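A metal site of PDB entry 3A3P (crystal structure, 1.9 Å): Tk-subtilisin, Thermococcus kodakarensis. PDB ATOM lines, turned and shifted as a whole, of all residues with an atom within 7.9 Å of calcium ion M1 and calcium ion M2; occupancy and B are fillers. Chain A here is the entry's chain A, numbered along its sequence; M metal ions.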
ATOM      1  N   ALA A 142     -15.177  -4.655 -12.815  1.00  0.00           N
ATOM      2  CA  ALA A 142     -14.303  -4.891 -11.659  1.00  0.00           C
ATOM      3  C   ALA A 142     -15.106  -4.848 -10.349  1.00  0.00           C
ATOM      4  O   ALA A 142     -15.016  -5.783  -9.538  1.00  0.00           O
ATOM      5  CB  ALA A 142     -13.158  -3.860 -11.606  1.00  0.00           C
ATOM      6  N   ASP A 143     -15.886  -3.764 -10.152  1.00  0.00           N
ATOM      7  CA  ASP A 143     -16.558  -3.487  -8.878  1.00  0.00           C
ATOM      8  C   ASP A 143     -17.993  -3.111  -9.176  1.00  0.00           C
ATOM      9  O   ASP A 143     -18.332  -1.942  -9.291  1.00  0.00           O
ATOM     10  CB  ASP A 143     -15.802  -2.368  -8.128  1.00  0.00           C
ATOM     11  CG  ASP A 143     -16.428  -1.980  -6.759  1.00  0.00           C
ATOM     12  OD1 ASP A 143     -17.230  -2.740  -6.157  1.00  0.00           O
ATOM     13  OD2 ASP A 143     -16.081  -0.876  -6.256  1.00  0.00           O
ATOM     14  N   LYS A 144     -18.855  -4.105  -9.299  1.00  0.00           N
ATOM     15  CA  LYS A 144     -20.205  -3.851  -9.805  1.00  0.00           C
ATOM     16  C   LYS A 144     -21.091  -3.007  -8.865  1.00  0.00           C
ATOM     17  O   LYS A 144     -21.905  -2.218  -9.328  1.00  0.00           O
ATOM     18  CB  LYS A 144     -20.807  -5.177 -10.262  1.00  0.00           C
ATOM     19  CG  LYS A 144     -22.204  -5.552  -9.807  1.00  0.00           C
ATOM     20  CD  LYS A 144     -22.526  -6.944 -10.395  1.00  0.00           C
ATOM     21  CE  LYS A 144     -22.069  -7.072 -11.886  1.00  0.00           C
ATOM     22  NZ  LYS A 144     -23.030  -6.661 -13.012  1.00  0.00           N
ATOM     23  N   ASP A 145     -20.887  -3.130  -7.551  1.00  0.00           N
ATOM     24  CA  ASP A 145     -21.671  -2.345  -6.604  1.00  0.00           C
ATOM     25  C   ASP A 145     -20.923  -1.120  -6.118  1.00  0.00           C
ATOM     26  O   ASP A 145     -21.363  -0.459  -5.193  1.00  0.00           O
ATOM     27  CB  ASP A 145     -22.132  -3.186  -5.426  1.00  0.00           C
ATOM     28  CG  ASP A 145     -20.998  -3.878  -4.706  1.00  0.00           C
ATOM     29  OD1 ASP A 145     -21.282  -4.666  -3.782  1.00  0.00           O
ATOM     30  OD2 ASP A 145     -19.825  -3.651  -5.055  1.00  0.00           O
ATOM     31  N   GLY A 146     -19.764  -0.847  -6.700  1.00  0.00           N
ATOM     32  CA  GLY A 146     -19.067   0.429  -6.426  1.00  0.00           C
ATOM     33  C   GLY A 146     -18.616   0.720  -5.004  1.00  0.00           C
ATOM     34  O   GLY A 146     -18.412   1.896  -4.638  1.00  0.00           O
ATOM     35  N   ASP A 147     -18.396  -0.327  -4.187  1.00  0.00           N
ATOM     36  CA  ASP A 147     -18.013  -0.132  -2.791  1.00  0.00           C
ATOM     37  C   ASP A 147     -16.505  -0.215  -2.576  1.00  0.00           C
ATOM     38  O   ASP A 147     -16.029  -0.130  -1.450  1.00  0.00           O
ATOM     39  CB  ASP A 147     -18.746  -1.135  -1.867  1.00  0.00           C
ATOM     40  CG  ASP A 147     -18.594  -2.593  -2.322  1.00  0.00           C
ATOM     41  OD1 ASP A 147     -17.653  -2.887  -3.105  1.00  0.00           O
ATOM     42  OD2 ASP A 147     -19.428  -3.458  -1.912  1.00  0.00           O
ATOM     43  N   GLY A 148     -15.732  -0.341  -3.654  1.00  0.00           N
ATOM     44  CA  GLY A 148     -14.267  -0.401  -3.519  1.00  0.00           C
ATOM     45  C   GLY A 148     -13.755  -1.764  -3.071  1.00  0.00           C
ATOM     46  O   GLY A 148     -12.548  -1.921  -2.858  1.00  0.00           O
ATOM     47  N   ILE A 149     -14.647  -2.741  -2.893  1.00  0.00           N
ATOM     48  CA  ILE A 149     -14.215  -4.088  -2.510  1.00  0.00           C
ATOM     49  C   ILE A 149     -14.320  -4.954  -3.757  1.00  0.00           C
ATOM     50  O   ILE A 149     -15.357  -5.030  -4.381  1.00  0.00           O
ATOM     51  CB  ILE A 149     -15.065  -4.666  -1.372  1.00  0.00           C
ATOM     52  CG1 ILE A 149     -15.220  -3.618  -0.264  1.00  0.00           C
ATOM     53  CG2 ILE A 149     -14.487  -6.004  -0.862  1.00  0.00           C
ATOM     54  CD1 ILE A 149     -16.097  -4.042   0.812  1.00  0.00           C
ATOM     55  N   ILE A 150     -13.229  -5.614  -4.120  1.00  0.00           N
ATOM     56  CA  ILE A 150     -13.219  -6.396  -5.349  1.00  0.00           C
ATOM     57  C   ILE A 150     -12.972  -7.871  -5.023  1.00  0.00           C
ATOM     58  O   ILE A 150     -13.948  -8.645  -4.979  1.00  0.00           O
ATOM     59  CB  ILE A 150     -12.274  -5.769  -6.410  1.00  0.00           C
ATOM     60  CG1 ILE A 150     -12.742  -4.323  -6.752  1.00  0.00           C
ATOM     61  CG2 ILE A 150     -12.215  -6.674  -7.709  1.00  0.00           C
ATOM     62  CD1 ILE A 150     -11.787  -3.507  -7.580  1.00  0.00           C
ATOM     63  N   ALA A 151     -11.702  -8.276  -4.812  1.00  0.00           N
ATOM     64  CA  ALA A 151     -11.413  -9.603  -4.234  1.00  0.00           C
ATOM     65  C   ALA A 151     -12.168  -9.757  -2.920  1.00  0.00           C
ATOM     66  O   ALA A 151     -12.166  -8.884  -2.060  1.00  0.00           O
ATOM     67  CB  ALA A 151      -9.899  -9.789  -3.980  1.00  0.00           C
ATOM     68  N   GLY A 152     -12.837 -10.896  -2.764  1.00  0.00           N
ATOM     69  CA  GLY A 152     -13.556 -11.172  -1.526  1.00  0.00           C
ATOM     70  C   GLY A 152     -14.963 -10.594  -1.399  1.00  0.00           C
ATOM     71  O   GLY A 152     -15.620 -10.877  -0.398  1.00  0.00           O
ATOM     72  N   ASP A 153     -15.398  -9.771  -2.366  1.00  0.00           N
ATOM     73  CA  ASP A 153     -16.765  -9.228  -2.369  1.00  0.00           C
ATOM     74  C   ASP A 153     -17.683 -10.256  -3.007  1.00  0.00           C
ATOM     75  O   ASP A 153     -17.532 -10.550  -4.199  1.00  0.00           O
ATOM     76  CB  ASP A 153     -16.851  -7.897  -3.127  1.00  0.00           C
ATOM     77  CG  ASP A 153     -18.230  -7.232  -2.972  1.00  0.00           C
ATOM     78  OD1 ASP A 153     -18.355  -6.017  -3.173  1.00  0.00           O
ATOM     79  OD2 ASP A 153     -19.206  -7.945  -2.687  1.00  0.00           O
ATOM     80  N   PRO A 154     -18.626 -10.820  -2.236  1.00  0.00           N
ATOM     81  CA  PRO A 154     -19.468 -11.851  -2.854  1.00  0.00           C
ATOM     82  C   PRO A 154     -20.387 -11.317  -3.929  1.00  0.00           C
ATOM     83  O   PRO A 154     -20.961 -12.094  -4.680  1.00  0.00           O
ATOM     84  CB  PRO A 154     -20.269 -12.416  -1.677  1.00  0.00           C
ATOM     85  CG  PRO A 154     -20.263 -11.290  -0.639  1.00  0.00           C
ATOM     86  CD  PRO A 154     -18.913 -10.649  -0.792  1.00  0.00           C
ATOM     87  N   ASP A 155     -20.530 -10.006  -4.034  1.00  0.00           N
ATOM     88  CA  ASP A 155     -21.303  -9.411  -5.125  1.00  0.00           C
ATOM     89  C   ASP A 155     -20.544  -9.386  -6.448  1.00  0.00           C
ATOM     90  O   ASP A 155     -21.170  -9.366  -7.510  1.00  0.00           O
ATOM     91  CB  ASP A 155     -21.776  -7.997  -4.772  1.00  0.00           C
ATOM     92  CG  ASP A 155     -22.791  -7.445  -5.764  1.00  0.00           C
ATOM     93  OD1 ASP A 155     -22.514  -6.382  -6.389  1.00  0.00           O
ATOM     94  OD2 ASP A 155     -23.849  -8.102  -5.939  1.00  0.00           O
ATOM     95  N   ASP A 156     -19.202  -9.413  -6.399  1.00  0.00           N
ATOM     96  CA  ASP A 156     -18.361  -9.367  -7.582  1.00  0.00           C
ATOM     97  C   ASP A 156     -17.820 -10.754  -7.879  1.00  0.00           C
ATOM     98  O   ASP A 156     -18.045 -11.679  -7.098  1.00  0.00           O
ATOM     99  CB  ASP A 156     -17.222  -8.379  -7.385  1.00  0.00           C
ATOM    100  CG  ASP A 156     -17.685  -6.947  -7.494  1.00  0.00           C
ATOM    101  OD1 ASP A 156     -18.187  -6.582  -8.581  1.00  0.00           O
ATOM    102  OD2 ASP A 156     -17.554  -6.198  -6.502  1.00  0.00           O
ATOM    103  N   ASP A 157     -17.063 -10.879  -8.976  1.00  0.00           N
ATOM    104  CA  ASP A 157     -16.547 -12.172  -9.408  1.00  0.00           C
ATOM    105  C   ASP A 157     -15.056 -12.177  -9.698  1.00  0.00           C
ATOM    106  O   ASP A 157     -14.564 -12.987 -10.501  1.00  0.00           O
ATOM    107  CB  ASP A 157     -17.313 -12.642 -10.637  1.00  0.00           C
ATOM    108  CG  ASP A 157     -17.227 -11.662 -11.787  1.00  0.00           C
ATOM    109  OD1 ASP A 157     -17.911 -11.934 -12.806  1.00  0.00           O
ATOM    110  OD2 ASP A 157     -16.515 -10.597 -11.697  1.00  0.00           O
HETATM  111 CA    CA M   1     -19.953  -5.166  -2.367  1.00  0.00          CA
HETATM  112 CA    CA M   2     -17.595  -4.536  -4.886  1.00  0.00          CA
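Of the 16 residues printed, 6 come within 4 Å of calcium ion M2.
OD1 of Asp 143 binds calcium ion M2 (2.2 Å). Calcium ion M2 is bound by OD2 of Asp 156, at 2.3 Å. The backbone carbonyl oxygen (O) of Ile 149 is bound to calcium ion M2. The side-chain carboxylate (OD1) of Asp 153 is bound to calcium ion M2. The side-chain carboxylate (OD2) of Asp 145 is bound to calcium ion M2, at 2.4 Å. OD1 of Asp 147 is bound to calcium ion M2 (2.4 Å).
Three residues have an atom within 4 Å of calcium ion M1: Asp 145, Asp 147 and Asp 153. The nearest printed residue that does not touch calcium ion M1 is Asp 155 (4.1 Å).
The backbone NH (N) of Asp 155 sits close to the side-chain carboxylate (OD2) of Asp 153 (2.8 Å). OD1 of Asp 143 sits close to N of Gly 146, at 3.2 Å. OD2 of Asp 143 is in hydrogen-bond range of N of Gly 148 (2.7 Å). N of Lys 144 lies within hydrogen-bond range of OD1 of Asp 156.
The side-chain carboxylate (OD2) of Asp 147 binds calcium ion M1. Calcium ion M1 is bound by the side-chain carboxylate (OD1) of Asp 153, 2.0 Å away. Calcium ion M1 is bound by the side-chain carboxylate (OD1) of Asp 145, at 2.0 Å. The side-chain carboxylate (OD2) of Asp 153 binds calcium ion M1, 2.9 Å away. Calcium ion M1 has four donor atoms within binding distance. Slightly farther from calcium ion M1 lies OD2 of Asp 145 (3.1 Å).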
